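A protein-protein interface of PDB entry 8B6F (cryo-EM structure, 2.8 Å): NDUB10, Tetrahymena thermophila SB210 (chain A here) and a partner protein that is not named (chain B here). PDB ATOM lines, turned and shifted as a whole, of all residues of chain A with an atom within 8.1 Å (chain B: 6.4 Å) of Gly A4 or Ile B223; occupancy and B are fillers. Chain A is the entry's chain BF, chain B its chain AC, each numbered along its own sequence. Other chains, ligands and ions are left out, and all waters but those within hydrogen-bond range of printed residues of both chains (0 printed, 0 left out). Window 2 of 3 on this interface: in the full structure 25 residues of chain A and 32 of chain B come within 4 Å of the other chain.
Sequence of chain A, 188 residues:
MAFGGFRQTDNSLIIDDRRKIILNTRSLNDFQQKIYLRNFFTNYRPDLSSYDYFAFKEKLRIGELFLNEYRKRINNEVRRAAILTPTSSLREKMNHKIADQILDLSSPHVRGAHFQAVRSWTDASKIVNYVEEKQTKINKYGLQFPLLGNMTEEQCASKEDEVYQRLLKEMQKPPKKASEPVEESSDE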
ATOM      1  N   ALA A   2      27.340  19.056  -2.283  1.00  0.00           N
ATOM      2  CA  ALA A   2      28.302  20.115  -2.694  1.00  0.00           C
ATOM      3  C   ALA A   2      27.893  21.477  -2.147  1.00  0.00           C
ATOM      4  O   ALA A   2      26.713  21.819  -2.144  1.00  0.00           O
ATOM      5  CB  ALA A   2      28.402  20.169  -4.201  1.00  0.00           C
ATOM      6  N   PHE A   3      28.871  22.251  -1.684  1.00  0.00           N
ATOM      7  CA  PHE A   3      28.589  23.591  -1.193  1.00  0.00           C
ATOM      8  C   PHE A   3      28.129  24.491  -2.332  1.00  0.00           C
ATOM      9  O   PHE A   3      28.512  24.315  -3.490  1.00  0.00           O
ATOM     10  CB  PHE A   3      29.828  24.203  -0.533  1.00  0.00           C
ATOM     11  CG  PHE A   3      30.131  23.663   0.840  1.00  0.00           C
ATOM     12  CD1 PHE A   3      29.113  23.359   1.730  1.00  0.00           C
ATOM     13  CD2 PHE A   3      31.441  23.472   1.242  1.00  0.00           C
ATOM     14  CE1 PHE A   3      29.396  22.873   2.989  1.00  0.00           C
ATOM     15  CE2 PHE A   3      31.730  22.987   2.499  1.00  0.00           C
ATOM     16  CZ  PHE A   3      30.705  22.686   3.374  1.00  0.00           C
ATOM     17  N   GLY A   4      27.294  25.467  -1.986  1.00  0.00           N
ATOM     18  CA  GLY A   4      26.794  26.422  -2.953  1.00  0.00           C
ATOM     19  C   GLY A   4      27.029  27.852  -2.519  1.00  0.00           C
ATOM     20  O   GLY A   4      27.912  28.120  -1.700  1.00  0.00           O
ATOM     21  N   GLY A   5      26.249  28.784  -3.063  1.00  0.00           N
ATOM     22  CA  GLY A   5      26.390  30.181  -2.709  1.00  0.00           C
ATOM     23  C   GLY A   5      25.067  30.905  -2.814  1.00  0.00           C
ATOM     24  O   GLY A   5      24.065  30.357  -3.276  1.00  0.00           O
ATOM     25  N   PHE A   6      25.080  32.157  -2.369  1.00  0.00           N
ATOM     26  CA  PHE A   6      23.913  33.026  -2.404  1.00  0.00           C
ATOM     27  C   PHE A   6      24.225  34.210  -3.307  1.00  0.00           C
ATOM     28  O   PHE A   6      25.298  34.811  -3.198  1.00  0.00           O
ATOM     29  CB  PHE A   6      23.542  33.502  -0.997  1.00  0.00           C
ATOM     30  CG  PHE A   6      22.167  34.096  -0.897  1.00  0.00           C
ATOM     31  CD1 PHE A   6      21.937  35.415  -1.246  1.00  0.00           C
ATOM     32  CD2 PHE A   6      21.108  33.336  -0.430  1.00  0.00           C
ATOM     33  CE1 PHE A   6      20.672  35.963  -1.146  1.00  0.00           C
ATOM     34  CE2 PHE A   6      19.842  33.876  -0.327  1.00  0.00           C
ATOM     35  CZ  PHE A   6      19.623  35.192  -0.684  1.00  0.00           C
ATOM     36  N   ARG A   7      23.292  34.536  -4.195  1.00  0.00           N
ATOM     37  CA  ARG A   7      23.509  35.610  -5.151  1.00  0.00           C
ATOM     38  C   ARG A   7      23.824  36.910  -4.424  1.00  0.00           C
ATOM     39  O   ARG A   7      23.186  37.254  -3.426  1.00  0.00           O
ATOM     40  CB  ARG A   7      22.274  35.786  -6.036  1.00  0.00           C
ATOM     41  CG  ARG A   7      22.421  36.843  -7.123  1.00  0.00           C
ATOM     42  CD  ARG A   7      23.472  36.461  -8.154  1.00  0.00           C
ATOM     43  NE  ARG A   7      23.130  35.228  -8.854  1.00  0.00           N
ATOM     44  CZ  ARG A   7      22.373  35.166  -9.941  1.00  0.00           C
ATOM     45  NH1 ARG A   7      21.849  36.252 -10.484  1.00  0.00           N
ATOM     46  NH2 ARG A   7      22.136  33.982 -10.499  1.00  0.00           N
ATOM     47  N   ASN A  29      30.001  33.360  -9.044  1.00  0.00           N
ATOM     48  CA  ASN A  29      29.274  32.107  -8.906  1.00  0.00           C
ATOM     49  C   ASN A  29      29.611  31.490  -7.549  1.00  0.00           C
ATOM     50  O   ASN A  29      30.248  32.116  -6.700  1.00  0.00           O
ATOM     51  CB  ASN A  29      29.588  31.172 -10.076  1.00  0.00           C
ATOM     52  CG  ASN A  29      31.050  30.785 -10.147  1.00  0.00           C
ATOM     53  OD1 ASN A  29      31.765  30.813  -9.150  1.00  0.00           O
ATOM     54  ND2 ASN A  29      31.501  30.411 -11.338  1.00  0.00           N
ATOM     55  N   ASP A  30      29.186  30.246  -7.327  1.00  0.00           N
ATOM     56  CA  ASP A  30      29.368  29.627  -6.017  1.00  0.00           C
ATOM     57  C   ASP A  30      30.845  29.435  -5.692  1.00  0.00           C
ATOM     58  O   ASP A  30      31.300  29.783  -4.598  1.00  0.00           O
ATOM     59  CB  ASP A  30      28.627  28.292  -5.965  1.00  0.00           C
ATOM     60  CG  ASP A  30      27.151  28.436  -6.277  1.00  0.00           C
ATOM     61  OD1 ASP A  30      26.812  28.680  -7.454  1.00  0.00           O
ATOM     62  OD2 ASP A  30      26.331  28.311  -5.345  1.00  0.00           O
ATOM     63  N   PHE A  31      31.609  28.868  -6.627  1.00  0.00           N
ATOM     64  CA  PHE A  31      33.022  28.619  -6.356  1.00  0.00           C
ATOM     65  C   PHE A  31      33.801  29.921  -6.211  1.00  0.00           C
ATOM     66  O   PHE A  31      34.655  30.044  -5.327  1.00  0.00           O
ATOM     67  CB  PHE A  31      33.628  27.758  -7.460  1.00  0.00           C
ATOM     68  CG  PHE A  31      35.114  27.609  -7.351  1.00  0.00           C
ATOM     69  CD1 PHE A  31      35.678  26.946  -6.276  1.00  0.00           C
ATOM     70  CD2 PHE A  31      35.948  28.136  -8.321  1.00  0.00           C
ATOM     71  CE1 PHE A  31      37.044  26.810  -6.170  1.00  0.00           C
ATOM     72  CE2 PHE A  31      37.316  28.005  -8.221  1.00  0.00           C
ATOM     73  CZ  PHE A  31      37.866  27.341  -7.143  1.00  0.00           C
ATOM     74  N   GLN A  33      32.610  32.776  -5.189  1.00  0.00           N
ATOM     75  CA  GLN A  33      32.252  33.303  -3.878  1.00  0.00           C
ATOM     76  C   GLN A  33      33.049  32.608  -2.782  1.00  0.00           C
ATOM     77  O   GLN A  33      33.580  33.260  -1.877  1.00  0.00           O
ATOM     78  CB  GLN A  33      30.752  33.137  -3.635  1.00  0.00           C
ATOM     79  CG  GLN A  33      29.884  34.075  -4.444  1.00  0.00           C
ATOM     80  CD  GLN A  33      28.417  33.726  -4.343  1.00  0.00           C
ATOM     81  OE1 GLN A  33      27.983  33.097  -3.382  1.00  0.00           O
ATOM     82  NE2 GLN A  33      27.643  34.133  -5.339  1.00  0.00           N
ATOM     83  N   LYS A  34      33.152  31.281  -2.855  1.00  0.00           N
ATOM     84  CA  LYS A  34      33.933  30.543  -1.868  1.00  0.00           C
ATOM     85  C   LYS A  34      35.382  31.013  -1.853  1.00  0.00           C
ATOM     86  O   LYS A  34      35.974  31.184  -0.781  1.00  0.00           O
ATOM     87  CB  LYS A  34      33.854  29.044  -2.172  1.00  0.00           C
ATOM     88  CG  LYS A  34      34.858  28.168  -1.427  1.00  0.00           C
ATOM     89  CD  LYS A  34      34.640  28.184   0.077  1.00  0.00           C
ATOM     90  CE  LYS A  34      33.402  27.392   0.464  1.00  0.00           C
ATOM     91  NZ  LYS A  34      33.265  27.275   1.942  1.00  0.00           N
ATOM     92  N   ARG A  38      34.016  34.477   1.972  1.00  0.00           N
ATOM     93  CA  ARG A  38      33.931  33.303   2.833  1.00  0.00           C
ATOM     94  C   ARG A  38      35.289  32.701   3.166  1.00  0.00           C
ATOM     95  O   ARG A  38      35.339  31.688   3.870  1.00  0.00           O
ATOM     96  CB  ARG A  38      33.062  32.198   2.215  1.00  0.00           C
ATOM     97  CG  ARG A  38      31.672  32.650   1.808  1.00  0.00           C
ATOM     98  CD  ARG A  38      30.835  31.475   1.333  1.00  0.00           C
ATOM     99  NE  ARG A  38      29.406  31.748   1.436  1.00  0.00           N
ATOM    100  CZ  ARG A  38      28.658  32.257   0.467  1.00  0.00           C
ATOM    101  NH1 ARG A  38      29.167  32.566  -0.713  1.00  0.00           N
ATOM    102  NH2 ARG A  38      27.364  32.462   0.689  1.00  0.00           N
ATOM    103  N   SER B 218      16.098  27.178   5.760  1.00  0.00           N
ATOM    104  CA  SER B 218      16.167  27.182   4.305  1.00  0.00           C
ATOM    105  C   SER B 218      17.403  27.926   3.818  1.00  0.00           C
ATOM    106  O   SER B 218      18.060  27.494   2.864  1.00  0.00           O
ATOM    107  CB  SER B 218      14.898  27.805   3.729  1.00  0.00           C
ATOM    108  OG  SER B 218      13.751  27.138   4.225  1.00  0.00           O
ATOM    109  N   TYR B 219      17.730  29.052   4.451  1.00  0.00           N
ATOM    110  CA  TYR B 219      18.952  29.764   4.096  1.00  0.00           C
ATOM    111  C   TYR B 219      20.173  28.873   4.283  1.00  0.00           C
ATOM    112  O   TYR B 219      21.056  28.819   3.421  1.00  0.00           O
ATOM    113  CB  TYR B 219      19.080  31.031   4.944  1.00  0.00           C
ATOM    114  CG  TYR B 219      18.667  32.300   4.238  1.00  0.00           C
ATOM    115  CD1 TYR B 219      17.348  32.733   4.263  1.00  0.00           C
ATOM    116  CD2 TYR B 219      19.597  33.071   3.557  1.00  0.00           C
ATOM    117  CE1 TYR B 219      16.965  33.895   3.622  1.00  0.00           C
ATOM    118  CE2 TYR B 219      19.225  34.234   2.914  1.00  0.00           C
ATOM    119  CZ  TYR B 219      17.908  34.642   2.950  1.00  0.00           C
ATOM    120  OH  TYR B 219      17.532  35.799   2.311  1.00  0.00           O
ATOM    121  N   ILE B 220      20.240  28.166   5.411  1.00  0.00           N
ATOM    122  CA  ILE B 220      21.405  27.333   5.698  1.00  0.00           C
ATOM    123  C   ILE B 220      21.485  26.171   4.715  1.00  0.00           C
ATOM    124  O   ILE B 220      22.555  25.867   4.175  1.00  0.00           O
ATOM    125  CB  ILE B 220      21.362  26.842   7.158  1.00  0.00           C
ATOM    126  CG1 ILE B 220      21.579  28.018   8.114  1.00  0.00           C
ATOM    127  CG2 ILE B 220      22.418  25.768   7.402  1.00  0.00           C
ATOM    128  CD1 ILE B 220      21.354  27.684   9.576  1.00  0.00           C
ATOM    129  N   ILE B 221      20.359  25.498   4.472  1.00  0.00           N
ATOM    130  CA  ILE B 221      20.377  24.293   3.649  1.00  0.00           C
ATOM    131  C   ILE B 221      20.625  24.639   2.187  1.00  0.00           C
ATOM    132  O   ILE B 221      21.415  23.979   1.502  1.00  0.00           O
ATOM    133  CB  ILE B 221      19.069  23.502   3.831  1.00  0.00           C
ATOM    134  CG1 ILE B 221      19.076  22.794   5.189  1.00  0.00           C
ATOM    135  CG2 ILE B 221      18.871  22.498   2.696  1.00  0.00           C
ATOM    136  CD1 ILE B 221      17.771  22.120   5.549  1.00  0.00           C
ATOM    137  N   SER B 222      19.940  25.662   1.675  1.00  0.00           N
ATOM    138  CA  SER B 222      20.120  26.024   0.273  1.00  0.00           C
ATOM    139  C   SER B 222      21.546  26.478  -0.003  1.00  0.00           C
ATOM    140  O   SER B 222      22.136  26.108  -1.024  1.00  0.00           O
ATOM    141  CB  SER B 222      19.125  27.113  -0.119  1.00  0.00           C
ATOM    142  OG  SER B 222      17.798  26.632  -0.025  1.00  0.00           O
ATOM    143  N   ILE B 223      22.116  27.284   0.892  1.00  0.00           N
ATOM    144  CA  ILE B 223      23.489  27.748   0.713  1.00  0.00           C
ATOM    145  C   ILE B 223      24.463  26.596   0.919  1.00  0.00           C
ATOM    146  O   ILE B 223      25.265  26.269   0.038  1.00  0.00           O
ATOM    147  CB  ILE B 223      23.786  28.919   1.666  1.00  0.00           C
ATOM    148  CG1 ILE B 223      22.843  30.089   1.373  1.00  0.00           C
ATOM    149  CG2 ILE B 223      25.236  29.363   1.532  1.00  0.00           C
ATOM    150  CD1 ILE B 223      22.888  31.192   2.409  1.00  0.00           C
ATOM    151  N   THR B 224      24.401  25.963   2.085  1.00  0.00           N
ATOM    152  CA  THR B 224      25.199  24.781   2.389  1.00  0.00           C
ATOM    153  C   THR B 224      24.313  23.561   2.201  1.00  0.00           C
ATOM    154  O   THR B 224      23.365  23.350   2.965  1.00  0.00           O
ATOM    155  CB  THR B 224      25.747  24.830   3.813  1.00  0.00           C
ATOM    156  OG1 THR B 224      24.665  24.734   4.748  1.00  0.00           O
ATOM    157  CG2 THR B 224      26.499  26.119   4.045  1.00  0.00           C
ATOM    158  N   ASN B 225      24.630  22.746   1.196  1.00  0.00           N
ATOM    159  CA  ASN B 225      23.835  21.557   0.928  1.00  0.00           C
ATOM    160  C   ASN B 225      23.980  20.507   2.019  1.00  0.00           C
ATOM    161  O   ASN B 225      23.231  19.525   2.016  1.00  0.00           O
ATOM    162  CB  ASN B 225      24.232  20.971  -0.427  1.00  0.00           C
ATOM    163  CG  ASN B 225      23.308  19.863  -0.872  1.00  0.00           C
ATOM    164  OD1 ASN B 225      22.168  19.774  -0.421  1.00  0.00           O
ATOM    165  ND2 ASN B 225      23.791  19.014  -1.767  1.00  0.00           N
ATOM    166  N   THR B 226      24.907  20.696   2.953  1.00  0.00           N
ATOM    167  CA  THR B 226      25.142  19.723   4.007  1.00  0.00           C
ATOM    168  C   THR B 226      23.957  19.662   4.967  1.00  0.00           C
ATOM    169  O   THR B 226      23.122  20.567   5.034  1.00  0.00           O
ATOM    170  CB  THR B 226      26.408  20.076   4.792  1.00  0.00           C
ATOM    171  OG1 THR B 226      26.216  21.311   5.494  1.00  0.00           O
ATOM    172  CG2 THR B 226      27.596  20.195   3.863  1.00  0.00           C
ATOM    173  N   PHE B 235      32.423  25.753   5.962  1.00  0.00           N
ATOM    174  CA  PHE B 235      31.729  26.760   5.172  1.00  0.00           C
ATOM    175  C   PHE B 235      31.492  27.985   6.039  1.00  0.00           C
ATOM    176  O   PHE B 235      30.997  27.864   7.163  1.00  0.00           O
ATOM    177  CB  PHE B 235      30.400  26.223   4.636  1.00  0.00           C
ATOM    178  CG  PHE B 235      29.762  27.109   3.610  1.00  0.00           C
ATOM    179  CD1 PHE B 235      28.961  28.171   3.990  1.00  0.00           C
ATOM    180  CD2 PHE B 235      29.967  26.879   2.261  1.00  0.00           C
ATOM    181  CE1 PHE B 235      28.374  28.983   3.046  1.00  0.00           C
ATOM    182  CE2 PHE B 235      29.383  27.686   1.311  1.00  0.00           C
ATOM    183  CZ  PHE B 235      28.586  28.741   1.705  1.00  0.00           C
ATOM    184  N   PHE B 237      29.664  31.746   6.308  1.00  0.00           N
ATOM    185  CA  PHE B 237      28.643  32.636   5.779  1.00  0.00           C
ATOM    186  C   PHE B 237      29.149  34.072   5.761  1.00  0.00           C
ATOM    187  O   PHE B 237      29.806  34.525   6.701  1.00  0.00           O
ATOM    188  CB  PHE B 237      27.368  32.548   6.619  1.00  0.00           C
ATOM    189  CG  PHE B 237      26.656  31.234   6.503  1.00  0.00           C
ATOM    190  CD1 PHE B 237      26.994  30.172   7.324  1.00  0.00           C
ATOM    191  CD2 PHE B 237      25.641  31.062   5.577  1.00  0.00           C
ATOM    192  CE1 PHE B 237      26.338  28.960   7.220  1.00  0.00           C
ATOM    193  CE2 PHE B 237      24.980  29.855   5.467  1.00  0.00           C
ATOM    194  CZ  PHE B 237      25.329  28.802   6.290  1.00  0.00           C
ATOM    195  N   GLU B 241      24.607  37.286   5.183  1.00  0.00           N
ATOM    196  CA  GLU B 241      23.929  36.021   5.436  1.00  0.00           C
ATOM    197  C   GLU B 241      23.922  35.696   6.922  1.00  0.00           C
ATOM    198  O   GLU B 241      22.907  35.247   7.465  1.00  0.00           O
ATOM    199  CB  GLU B 241      24.601  34.899   4.646  1.00  0.00           C
ATOM    200  CG  GLU B 241      24.618  35.130   3.146  1.00  0.00           C
ATOM    201  CD  GLU B 241      25.461  34.107   2.413  1.00  0.00           C
ATOM    202  OE1 GLU B 241      25.927  33.146   3.059  1.00  0.00           O
ATOM    203  OE2 GLU B 241      25.663  34.265   1.192  1.00  0.00           O
ATOM    204  N   ILE B 245      20.658  35.306   9.325  1.00  0.00           N
ATOM    205  CA  ILE B 245      20.396  34.037   9.998  1.00  0.00           C
ATOM    206  C   ILE B 245      20.210  34.252  11.495  1.00  0.00           C
ATOM    207  O   ILE B 245      19.281  33.712  12.104  1.00  0.00           O
ATOM    208  CB  ILE B 245      21.525  33.033   9.703  1.00  0.00           C
ATOM    209  CG1 ILE B 245      21.437  32.562   8.248  1.00  0.00           C
ATOM    210  CG2 ILE B 245      21.462  31.839  10.657  1.00  0.00           C
ATOM    211  CD1 ILE B 245      22.615  31.733   7.790  1.00  0.00           C
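O of Ile B223 lies within hydrogen-bond range of N of Gly A4, at 3.0 Å. The side-chain carboxylate of Glu B241 is in salt-bridge range of the guanidinium group of Arg A38, 2.5 Å away.
Hydrophobic or aromatic side chains of chain A within 4 Å of the printed part of chain B: Phe A3 and Phe A6. Hydrophobic or aromatic side chains of chain B within 4 Å of the printed part of chain A: Tyr B219, Ile B223 and Phe B235.
Printed residues of chain B within 4 Å of Ala A2: Asn B225 (3.1 Å). Gly A4 touches just these residues of chain B: Ile B223 (3.0 Å) and Phe B235 (3.4 Å). Of the printed residues of chain B, Phe A6 touches Tyr B219, Ile B223 and Glu B241. Of the printed residues of chain B, Lys A34 touches Phe B235 (3.3 Å). Of the printed residues of chain A, Tyr B219 touches Phe A6. Of chain A, only Gly A4 (3.0 Å), Phe A6 (3.98 Å) and Arg A38 (3.9 Å) come within 4 Å of Ile B223. Of the printed residues of chain A, Glu B241 touches Phe A6 and Arg A38. The nearest residue of chain B that does not touch Gly A4 is Thr B224 (4.9 Å). The nearest printed residue of chain A that does not touch Ile B223 is Gly A5 (4.1 Å).
The side-chain amide oxygen (OE1) of Gln A33 sits close to the backbone carbonyl oxygen (O) of Phe A6 (3.2 Å). OE1 of Gln A33 lies within hydrogen-bond range of NH1 of Arg A38 (3.0 Å).
Among the printed residues, pairs that only touch across the chains: Ala A2 with Asn B225, Phe A3 with Thr B226, Phe A3 with Phe B235, Gly A4 with Phe B235, Phe A6 with Tyr B219, Phe A6 with Ile B223, Phe A6 with Glu B241, Lys A34 with Phe B235, Arg A38 with Ile B223 and Arg A38 with Phe B235.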
